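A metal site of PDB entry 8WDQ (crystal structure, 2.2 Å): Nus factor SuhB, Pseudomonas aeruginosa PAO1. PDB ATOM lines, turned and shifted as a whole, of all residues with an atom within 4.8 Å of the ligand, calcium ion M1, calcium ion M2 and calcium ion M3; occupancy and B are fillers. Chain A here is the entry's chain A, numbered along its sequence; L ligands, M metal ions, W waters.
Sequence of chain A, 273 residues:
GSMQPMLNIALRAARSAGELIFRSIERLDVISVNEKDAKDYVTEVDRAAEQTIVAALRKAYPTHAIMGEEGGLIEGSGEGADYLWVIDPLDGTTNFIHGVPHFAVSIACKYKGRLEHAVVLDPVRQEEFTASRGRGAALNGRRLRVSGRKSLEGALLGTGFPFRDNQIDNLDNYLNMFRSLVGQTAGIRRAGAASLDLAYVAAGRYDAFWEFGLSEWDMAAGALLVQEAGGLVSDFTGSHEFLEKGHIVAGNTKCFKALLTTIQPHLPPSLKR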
ATOM      1  N   LYS A  36     -17.168  -3.631   1.109  1.00  0.00           N
ATOM      2  CA  LYS A  36     -16.145  -4.195   0.242  1.00  0.00           C
ATOM      3  C   LYS A  36     -15.736  -5.582   0.727  1.00  0.00           C
ATOM      4  O   LYS A  36     -15.667  -6.539  -0.060  1.00  0.00           O
ATOM      5  CB  LYS A  36     -14.928  -3.262   0.192  1.00  0.00           C
ATOM      6  CG  LYS A  36     -15.173  -1.959  -0.566  1.00  0.00           C
ATOM      7  CD  LYS A  36     -13.887  -1.153  -0.713  1.00  0.00           C
ATOM      8  CE  LYS A  36     -13.265  -0.852   0.636  1.00  0.00           C
ATOM      9  NZ  LYS A  36     -12.027  -0.029   0.507  1.00  0.00           N
ATOM     10  N   ASP A  40     -15.260  -4.292   6.330  1.00  0.00           N
ATOM     11  CA  ASP A  40     -14.591  -3.316   5.479  1.00  0.00           C
ATOM     12  C   ASP A  40     -15.679  -2.528   4.763  1.00  0.00           C
ATOM     13  O   ASP A  40     -16.268  -3.012   3.787  1.00  0.00           O
ATOM     14  CB  ASP A  40     -13.652  -4.011   4.509  1.00  0.00           C
ATOM     15  CG  ASP A  40     -12.678  -3.062   3.829  1.00  0.00           C
ATOM     16  OD1 ASP A  40     -12.217  -2.117   4.496  1.00  0.00           O
ATOM     17  OD2 ASP A  40     -12.380  -3.270   2.634  1.00  0.00           O
ATOM     18  N   ASP A  46     -16.818   8.158   1.295  1.00  0.00           N
ATOM     19  CA  ASP A  46     -15.488   7.744   0.865  1.00  0.00           C
ATOM     20  C   ASP A  46     -15.269   8.037  -0.619  1.00  0.00           C
ATOM     21  O   ASP A  46     -14.235   8.596  -1.006  1.00  0.00           O
ATOM     22  CB  ASP A  46     -15.270   6.248   1.145  1.00  0.00           C
ATOM     23  CG  ASP A  46     -15.386   5.900   2.621  1.00  0.00           C
ATOM     24  OD1 ASP A  46     -14.396   6.054   3.362  1.00  0.00           O
ATOM     25  OD2 ASP A  46     -16.469   5.442   3.031  1.00  0.00           O
ATOM     26  N   GLU A  69      -7.787   4.265  -2.388  1.00  0.00           N
ATOM     27  CA  GLU A  69      -8.364   3.082  -1.745  1.00  0.00           C
ATOM     28  C   GLU A  69      -9.593   2.597  -2.512  1.00  0.00           C
ATOM     29  O   GLU A  69      -9.730   1.401  -2.789  1.00  0.00           O
ATOM     30  CB  GLU A  69      -8.713   3.371  -0.289  1.00  0.00           C
ATOM     31  CG  GLU A  69      -9.726   2.385   0.273  1.00  0.00           C
ATOM     32  CD  GLU A  69      -9.741   2.297   1.789  1.00  0.00           C
ATOM     33  OE1 GLU A  69      -9.374   3.287   2.473  1.00  0.00           O
ATOM     34  OE2 GLU A  69     -10.122   1.224   2.306  1.00  0.00           O
ATOM     35  N   GLU A  70     -10.482   3.508  -2.883  1.00  0.00           N
ATOM     36  CA  GLU A  70     -11.694   3.094  -3.600  1.00  0.00           C
ATOM     37  C   GLU A  70     -11.413   2.816  -5.073  1.00  0.00           C
ATOM     38  O   GLU A  70     -11.937   1.839  -5.626  1.00  0.00           O
ATOM     39  CB  GLU A  70     -12.790   4.143  -3.458  1.00  0.00           C
ATOM     40  CG  GLU A  70     -13.013   4.689  -2.039  1.00  0.00           C
ATOM     41  CD  GLU A  70     -13.062   3.602  -0.972  1.00  0.00           C
ATOM     42  OE1 GLU A  70     -13.518   2.471  -1.254  1.00  0.00           O
ATOM     43  OE2 GLU A  70     -12.646   3.891   0.181  1.00  0.00           O
ATOM     44  N   ASP A  88      -5.851   7.569   1.023  1.00  0.00           N
ATOM     45  CA  ASP A  88      -7.001   7.102   1.779  1.00  0.00           C
ATOM     46  C   ASP A  88      -7.932   8.295   1.933  1.00  0.00           C
ATOM     47  O   ASP A  88      -7.652   9.196   2.737  1.00  0.00           O
ATOM     48  CB  ASP A  88      -6.610   6.553   3.148  1.00  0.00           C
ATOM     49  CG  ASP A  88      -7.747   5.772   3.805  1.00  0.00           C
ATOM     50  OD1 ASP A  88      -8.917   6.008   3.443  1.00  0.00           O
ATOM     51  OD2 ASP A  88      -7.466   4.972   4.711  1.00  0.00           O
ATOM     52  N   LEU A  90     -10.780   8.597   3.370  1.00  0.00           N
ATOM     53  CA  LEU A  90     -11.410   8.664   4.685  1.00  0.00           C
ATOM     54  C   LEU A  90     -10.856   7.496   5.502  1.00  0.00           C
ATOM     55  O   LEU A  90     -11.310   6.356   5.364  1.00  0.00           O
ATOM     56  CB  LEU A  90     -12.920   8.598   4.570  1.00  0.00           C
ATOM     57  CG  LEU A  90     -13.764   8.480   5.852  1.00  0.00           C
ATOM     58  CD1 LEU A  90     -13.287   9.439   6.936  1.00  0.00           C
ATOM     59  CD2 LEU A  90     -15.228   8.712   5.538  1.00  0.00           C
ATOM     60  N   ASP A  91      -9.865   7.777   6.337  1.00  0.00           N
ATOM     61  CA  ASP A  91      -9.305   6.762   7.231  1.00  0.00           C
ATOM     62  C   ASP A  91      -9.965   6.877   8.606  1.00  0.00           C
ATOM     63  O   ASP A  91      -9.920   7.937   9.228  1.00  0.00           O
ATOM     64  CB  ASP A  91      -7.783   6.879   7.282  1.00  0.00           C
ATOM     65  CG  ASP A  91      -7.137   5.894   8.241  1.00  0.00           C
ATOM     66  OD1 ASP A  91      -6.301   6.316   9.030  1.00  0.00           O
ATOM     67  OD2 ASP A  91      -7.545   4.736   8.341  1.00  0.00           O
ATOM     68  N   GLY A  92     -10.598   5.792   9.038  1.00  0.00           N
ATOM     69  CA  GLY A  92     -11.484   5.784  10.189  1.00  0.00           C
ATOM     70  C   GLY A  92     -12.959   5.635   9.816  1.00  0.00           C
ATOM     71  O   GLY A  92     -13.824   6.282  10.418  1.00  0.00           O
ATOM     72  N   THR A  93     -13.248   4.762   8.836  1.00  0.00           N
ATOM     73  CA  THR A  93     -14.598   4.665   8.269  1.00  0.00           C
ATOM     74  C   THR A  93     -15.604   4.139   9.283  1.00  0.00           C
ATOM     75  O   THR A  93     -16.766   4.571   9.300  1.00  0.00           O
ATOM     76  CB  THR A  93     -14.570   3.773   7.020  1.00  0.00           C
ATOM     77  OG1 THR A  93     -13.820   4.422   5.974  1.00  0.00           O
ATOM     78  CG2 THR A  93     -15.970   3.501   6.511  1.00  0.00           C
ATOM     79  N   THR A  94     -15.214   3.189  10.138  1.00  0.00           N
ATOM     80  CA  THR A  94     -16.148   2.671  11.127  1.00  0.00           C
ATOM     81  C   THR A  94     -16.486   3.729  12.171  1.00  0.00           C
ATOM     82  O   THR A  94     -17.657   3.921  12.526  1.00  0.00           O
ATOM     83  CB  THR A  94     -15.576   1.402  11.764  1.00  0.00           C
ATOM     84  OG1 THR A  94     -15.219   0.477  10.724  1.00  0.00           O
ATOM     85  CG2 THR A  94     -16.592   0.747  12.707  1.00  0.00           C
ATOM     86  N   GLY A 160      -3.575  -0.785  16.705  1.00  0.00           N
ATOM     87  CA  GLY A 160      -4.798  -1.158  16.005  1.00  0.00           C
ATOM     88  C   GLY A 160      -5.092  -2.621  16.209  1.00  0.00           C
ATOM     89  O   GLY A 160      -4.183  -3.453  16.197  1.00  0.00           O
ATOM     90  N   PHE A 161      -6.373  -2.936  16.383  1.00  0.00           N
ATOM     91  CA  PHE A 161      -6.797  -4.283  16.744  1.00  0.00           C
ATOM     92  C   PHE A 161      -6.960  -5.152  15.510  1.00  0.00           C
ATOM     93  O   PHE A 161      -7.469  -4.691  14.485  1.00  0.00           O
ATOM     94  CB  PHE A 161      -8.122  -4.247  17.524  1.00  0.00           C
ATOM     95  CG  PHE A 161      -8.037  -3.545  18.838  1.00  0.00           C
ATOM     96  CD1 PHE A 161      -6.843  -3.498  19.551  1.00  0.00           C
ATOM     97  CD2 PHE A 161      -9.169  -2.935  19.381  1.00  0.00           C
ATOM     98  CE1 PHE A 161      -6.779  -2.852  20.768  1.00  0.00           C
ATOM     99  CE2 PHE A 161      -9.099  -2.286  20.605  1.00  0.00           C
ATOM    100  CZ  PHE A 161      -7.910  -2.252  21.301  1.00  0.00           C
ATOM    101  N   PHE A 163      -9.105  -7.017  13.851  1.00  0.00           N
ATOM    102  CA  PHE A 163     -10.556  -7.194  13.952  1.00  0.00           C
ATOM    103  C   PHE A 163     -11.153  -8.016  12.807  1.00  0.00           C
ATOM    104  O   PHE A 163     -12.296  -8.451  12.931  1.00  0.00           O
ATOM    105  CB  PHE A 163     -11.246  -5.827  14.008  1.00  0.00           C
ATOM    106  CG  PHE A 163     -11.073  -5.011  12.750  1.00  0.00           C
ATOM    107  CD1 PHE A 163      -9.938  -4.251  12.559  1.00  0.00           C
ATOM    108  CD2 PHE A 163     -12.063  -5.002  11.773  1.00  0.00           C
ATOM    109  CE1 PHE A 163      -9.784  -3.491  11.402  1.00  0.00           C
ATOM    110  CE2 PHE A 163     -11.911  -4.259  10.613  1.00  0.00           C
ATOM    111  CZ  PHE A 163     -10.770  -3.495  10.429  1.00  0.00           C
ATOM    112  N   ARG A 164     -10.429  -8.221  11.717  1.00  0.00           N
ATOM    113  CA  ARG A 164     -10.974  -8.914  10.562  1.00  0.00           C
ATOM    114  C   ARG A 164     -11.082 -10.409  10.831  1.00  0.00           C
ATOM    115  O   ARG A 164     -10.335 -10.973  11.639  1.00  0.00           O
ATOM    116  CB  ARG A 164     -10.118  -8.669   9.322  1.00  0.00           C
ATOM    117  CG  ARG A 164     -10.025  -7.212   8.886  1.00  0.00           C
ATOM    118  CD  ARG A 164      -8.814  -6.993   7.983  1.00  0.00           C
ATOM    119  NE  ARG A 164      -8.573  -5.573   7.720  1.00  0.00           N
ATOM    120  CZ  ARG A 164      -7.948  -4.743   8.539  1.00  0.00           C
ATOM    121  NH1 ARG A 164      -7.453  -5.167   9.698  1.00  0.00           N
ATOM    122  NH2 ARG A 164      -7.800  -3.468   8.186  1.00  0.00           N
ATOM    123  N   ARG A 190      -6.429   2.790  21.304  1.00  0.00           N
ATOM    124  CA  ARG A 190      -6.919   2.322  20.007  1.00  0.00           C
ATOM    125  C   ARG A 190      -8.055   3.264  19.641  1.00  0.00           C
ATOM    126  O   ARG A 190      -9.217   3.022  19.972  1.00  0.00           O
ATOM    127  CB  ARG A 190      -7.369   0.863  20.062  1.00  0.00           C
ATOM    128  CG  ARG A 190      -7.429   0.179  18.689  1.00  0.00           C
ATOM    129  CD  ARG A 190      -8.748   0.464  17.967  1.00  0.00           C
ATOM    130  NE  ARG A 190      -8.958  -0.411  16.819  1.00  0.00           N
ATOM    131  CZ  ARG A 190      -8.408  -0.239  15.628  1.00  0.00           C
ATOM    132  NH1 ARG A 190      -7.576   0.765  15.388  1.00  0.00           N
ATOM    133  NH2 ARG A 190      -8.703  -1.085  14.641  1.00  0.00           N
ATOM    134  N   GLY A 192      -8.806   4.292  16.442  1.00  0.00           N
ATOM    135  CA  GLY A 192      -9.489   3.824  15.257  1.00  0.00           C
ATOM    136  C   GLY A 192      -9.144   4.496  13.946  1.00  0.00           C
ATOM    137  O   GLY A 192      -9.939   4.396  12.993  1.00  0.00           O
ATOM    138  N   ALA A 193      -7.999   5.161  13.835  1.00  0.00           N
ATOM    139  CA  ALA A 193      -7.567   5.733  12.554  1.00  0.00           C
ATOM    140  C   ALA A 193      -6.046   5.673  12.492  1.00  0.00           C
ATOM    141  O   ALA A 193      -5.366   6.486  13.115  1.00  0.00           O
ATOM    142  CB  ALA A 193      -8.079   7.160  12.381  1.00  0.00           C
ATOM    143  N   ALA A 194      -5.522   4.726  11.713  1.00  0.00           N
ATOM    144  CA  ALA A 194      -4.085   4.456  11.714  1.00  0.00           C
ATOM    145  C   ALA A 194      -3.269   5.668  11.272  1.00  0.00           C
ATOM    146  O   ALA A 194      -2.162   5.894  11.790  1.00  0.00           O
ATOM    147  CB  ALA A 194      -3.778   3.249  10.825  1.00  0.00           C
ATOM    148  N   SER A 195      -3.771   6.433  10.307  1.00  0.00           N
ATOM    149  CA  SER A 195      -3.032   7.613   9.863  1.00  0.00           C
ATOM    150  C   SER A 195      -2.856   8.605  10.998  1.00  0.00           C
ATOM    151  O   SER A 195      -1.798   9.235  11.136  1.00  0.00           O
ATOM    152  CB  SER A 195      -3.729   8.285   8.675  1.00  0.00           C
ATOM    153  OG  SER A 195      -5.030   8.713   9.030  1.00  0.00           O
ATOM    154  N   GLU A 211       0.926  -2.300  14.447  1.00  0.00           N
ATOM    155  CA  GLU A 211      -0.308  -2.862  13.906  1.00  0.00           C
ATOM    156  C   GLU A 211       0.050  -3.741  12.714  1.00  0.00           C
ATOM    157  O   GLU A 211       0.989  -3.433  11.979  1.00  0.00           O
ATOM    158  CB  GLU A 211      -1.303  -1.767  13.469  1.00  0.00           C
ATOM    159  CG  GLU A 211      -2.608  -2.316  12.898  1.00  0.00           C
ATOM    160  CD  GLU A 211      -3.706  -1.261  12.756  1.00  0.00           C
ATOM    161  OE1 GLU A 211      -3.431  -0.063  12.966  1.00  0.00           O
ATOM    162  OE2 GLU A 211      -4.855  -1.638  12.447  1.00  0.00           O
ATOM    163  N   LEU A 214      -2.580  -3.781   7.759  1.00  0.00           N
ATOM    164  CA  LEU A 214      -2.858  -2.483   7.160  1.00  0.00           C
ATOM    165  C   LEU A 214      -2.568  -2.495   5.663  1.00  0.00           C
ATOM    166  O   LEU A 214      -1.829  -3.342   5.141  1.00  0.00           O
ATOM    167  CB  LEU A 214      -2.010  -1.387   7.824  1.00  0.00           C
ATOM    168  CG  LEU A 214      -2.382  -0.992   9.249  1.00  0.00           C
ATOM    169  CD1 LEU A 214      -1.404   0.067   9.774  1.00  0.00           C
ATOM    170  CD2 LEU A 214      -3.816  -0.476   9.338  1.00  0.00           C
ATOM    171  N   ASP A 218      -3.182   3.319   4.257  1.00  0.00           N
ATOM    172  CA  ASP A 218      -3.290   3.564   5.693  1.00  0.00           C
ATOM    173  C   ASP A 218      -2.000   4.149   6.244  1.00  0.00           C
ATOM    174  O   ASP A 218      -2.028   4.975   7.172  1.00  0.00           O
ATOM    175  CB  ASP A 218      -3.619   2.263   6.445  1.00  0.00           C
ATOM    176  CG  ASP A 218      -4.911   1.614   5.982  1.00  0.00           C
ATOM    177  OD1 ASP A 218      -5.946   2.300   5.822  1.00  0.00           O
ATOM    178  OD2 ASP A 218      -4.885   0.380   5.765  1.00  0.00           O
HETATM  179  C1  LIG L   1      -7.963   1.611   8.824  1.00  0.00           C
HETATM  180  C2  LIG L   1      -8.191   2.401  10.128  1.00  0.00           C
HETATM  181  C3  LIG L   1      -8.153   1.599  11.435  1.00  0.00           C
HETATM  182  C4  LIG L   1      -7.246   0.380  11.287  1.00  0.00           C
HETATM  183  C5  LIG L   1      -7.837  -0.576  10.243  1.00  0.00           C
HETATM  184  C6  LIG L   1      -7.953   0.067   8.842  1.00  0.00           C
HETATM  185  P1  LIG L   1     -10.184   2.398   7.247  1.00  0.00           P
HETATM  186  O1  LIG L   1      -8.602   2.201   7.695  1.00  0.00           O
HETATM  187  O2  LIG L   1      -7.049   3.234  10.180  1.00  0.00           O
HETATM  188  O3  LIG L   1      -7.630   2.423  12.460  1.00  0.00           O
HETATM  189  O4  LIG L   1      -7.136  -0.281  12.531  1.00  0.00           O
HETATM  190  O5  LIG L   1      -6.969  -1.677  10.143  1.00  0.00           O
HETATM  191  O6  LIG L   1      -9.057  -0.448   8.135  1.00  0.00           O
HETATM  192  O7  LIG L   1     -10.990   3.198   8.247  1.00  0.00           O
HETATM  193  O8  LIG L   1     -10.079   3.184   5.965  1.00  0.00           O
HETATM  194  O9  LIG L   1     -10.868   1.076   6.946  1.00  0.00           O
HETATM  195 CA    CA M   1     -10.512   4.549   4.151  1.00  0.00          CA
HETATM  196 CA    CA M   2      -7.367   4.002   6.726  1.00  0.00          CA
HETATM  197 CA    CA M   3     -10.721   0.816   4.590  1.00  0.00          CA
HETATM  198  O   HOH W   1     -11.968  -0.705   8.212  1.00  0.00           O
HETATM  199  O   HOH W   2     -13.034   0.049   4.573  1.00  0.00           O
HETATM  200  O   HOH W   3     -11.115  -2.826   7.046  1.00  0.00           O
HETATM  201  O   HOH W   4      -9.993  -1.528   4.819  1.00  0.00           O
HETATM  202  O   HOH W   5      -8.263   1.007   4.391  1.00  0.00           O
HETATM  203  O   HOH W   6      -6.929  -1.286   5.821  1.00  0.00           O
HETATM  204  O   HOH W   7     -12.408   2.123  10.272  1.00  0.00           O
HETATM  205  O   HOH W   8     -12.173   5.188   2.537  1.00  0.00           O
HETATM  206  O   HOH W   9      -5.129   2.061  13.768  1.00  0.00           O
HETATM  207  O   HOH W  10      -5.953  -4.058  12.193  1.00  0.00           O
HETATM  208  O   HOH W  11     -12.309   2.813   4.377  1.00  0.00           O
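Merely in contact with the ligand: Leu 214 (3.5 Å) and Phe 163 (3.6 Å).
Hydrophobic or aromatic side chains within 4 Å of the ligand: Phe 163, Ala 194 and Leu 214.
OD2 of Asp 40 is in salt-bridge range of NZ of Lys 36, at 3.9 Å.
OD1 of Asp 91 lies within hydrogen-bond range of N of Ala 194.
OD1 of Asp 91 lies within hydrogen-bond range of OG of Ser 195.
OG1 of Thr 93 sits at hydrogen-bond distance from OD1 of Asp 46 (3.1 Å).
The side-chain hydroxyl (OG1) of Thr 93 sits close to the backbone carbonyl oxygen (O) of Leu 90, 3.2 Å away.
The side-chain carboxylate of Glu 69 sits close to the side-chain amino group of Lys 36.
Calcium ion M1 is bound by OD1 of Asp 88, O8 of the ligand, O of Leu 90, OE1 of Glu 69, water W8 and water W11.
Calcium ion M1 has six donor atoms within binding distance.
Slightly farther from calcium ion M1 lies the side-chain carboxylate (OD2) of Asp 88 (3.1 Å).
Water W8 bridges OD1 of Asp 46 (2.5 Å) and OE2 of Glu 70 (2.7 Å).
Water W7 lies within hydrogen-bond range of an oxygen (O7) of the ligand (2.7 Å), the backbone NH of Thr 94 (3.0 Å) and the backbone NH of Thr 93 (3.1 Å).
Water W9 lies within hydrogen-bond range of the side-chain carboxylate of Glu 211 (2.8 Å), an oxygen (O3) of the ligand (2.8 Å), the guanidinium group of Arg 190 (3.2 Å) and the backbone NH of Ala 194 (3.4 Å).
Water W6 lies within hydrogen-bond range of OD2 of Asp 218 (2.6 Å), O6 of the ligand (3.3 Å) and NH2 of Arg 164 (3.3 Å).
Water W10 lies within hydrogen-bond range of OE2 of Glu 211, O of Phe 161, NH1 of Arg 164 and O5 of the ligand.
Water W3 lies within hydrogen-bond range of OD1 of Asp 40 (2.9 Å) and O6 of the ligand (3.3 Å).
Three residues have an atom within 4 Å of calcium ion M2: Asp 88, Asp 91 and Asp 218.
The nearest printed residue that does not touch calcium ion M2 is Gly 92 (4.4 Å).
An oxygen (O4) of the ligand lies within hydrogen-bond range of the side-chain carboxylate (OE2) of Glu 211, 2.7 Å away.
The guanidinium group (NH2) of Arg 164 sits at hydrogen-bond distance from an oxygen (O5) of the ligand, at 2.8 Å.
An oxygen (O3) of the ligand sits at hydrogen-bond distance from the backbone NH of Ala 193 (3.1 Å).
O7 of the ligand lies within hydrogen-bond range of N of Gly 92 (2.7 Å).
An oxygen (O2) of the ligand sits at hydrogen-bond distance from the backbone NH (N) of Ala 194.
The backbone NH (N) of Thr 93 sits at hydrogen-bond distance from an oxygen (O7) of the ligand.
An oxygen (O3) of the ligand sits close to the backbone carbonyl oxygen of Gly 192 (3.1 Å).
NH2 of Arg 190 sits at hydrogen-bond distance from O4 of the ligand, 2.7 Å away.
O9 of the ligand is bound to calcium ion M3.
OE2 of Glu 69 binds calcium ion M3.
Water W2 is bound to calcium ion M3, 2.4 Å away.
Calcium ion M3 is bound by water W4, at 2.5 Å.
Water W5 is bound to calcium ion M3, at 2.5 Å.
Calcium ion M3 is bound by water W11, 2.6 Å away.
O8 of the ligand binds calcium ion M3, at 2.8 Å.
OD1 of Asp 40 touches calcium ion M3 (3.3 Å).
Two residues have an atom within 4 Å of calcium ion M3: Asp 40 and Glu 69.
The nearest printed residue that does not touch calcium ion M3 is Lys 36 (4.4 Å).
Merely in contact with calcium ion M1: Thr 93.
Five residues have an atom within 4 Å of calcium ion M1: Glu 69, Asp 88, Leu 90, Asp 91 and Thr 93.
The nearest printed residue that does not touch calcium ion M1 is Asp 46 (4.2 Å).
Calcium ion M2 is bound by the side-chain carboxylate (OD2) of Asp 91 (1.8 Å), the side-chain carboxylate (OD2) of Asp 88 (2.2 Å), an oxygen (O1) of the ligand (2.4 Å) and the side-chain carboxylate (OD1) of Asp 218 (2.4 Å).
Slightly farther from calcium ion M2 lies O8 of the ligand (2.9 Å).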
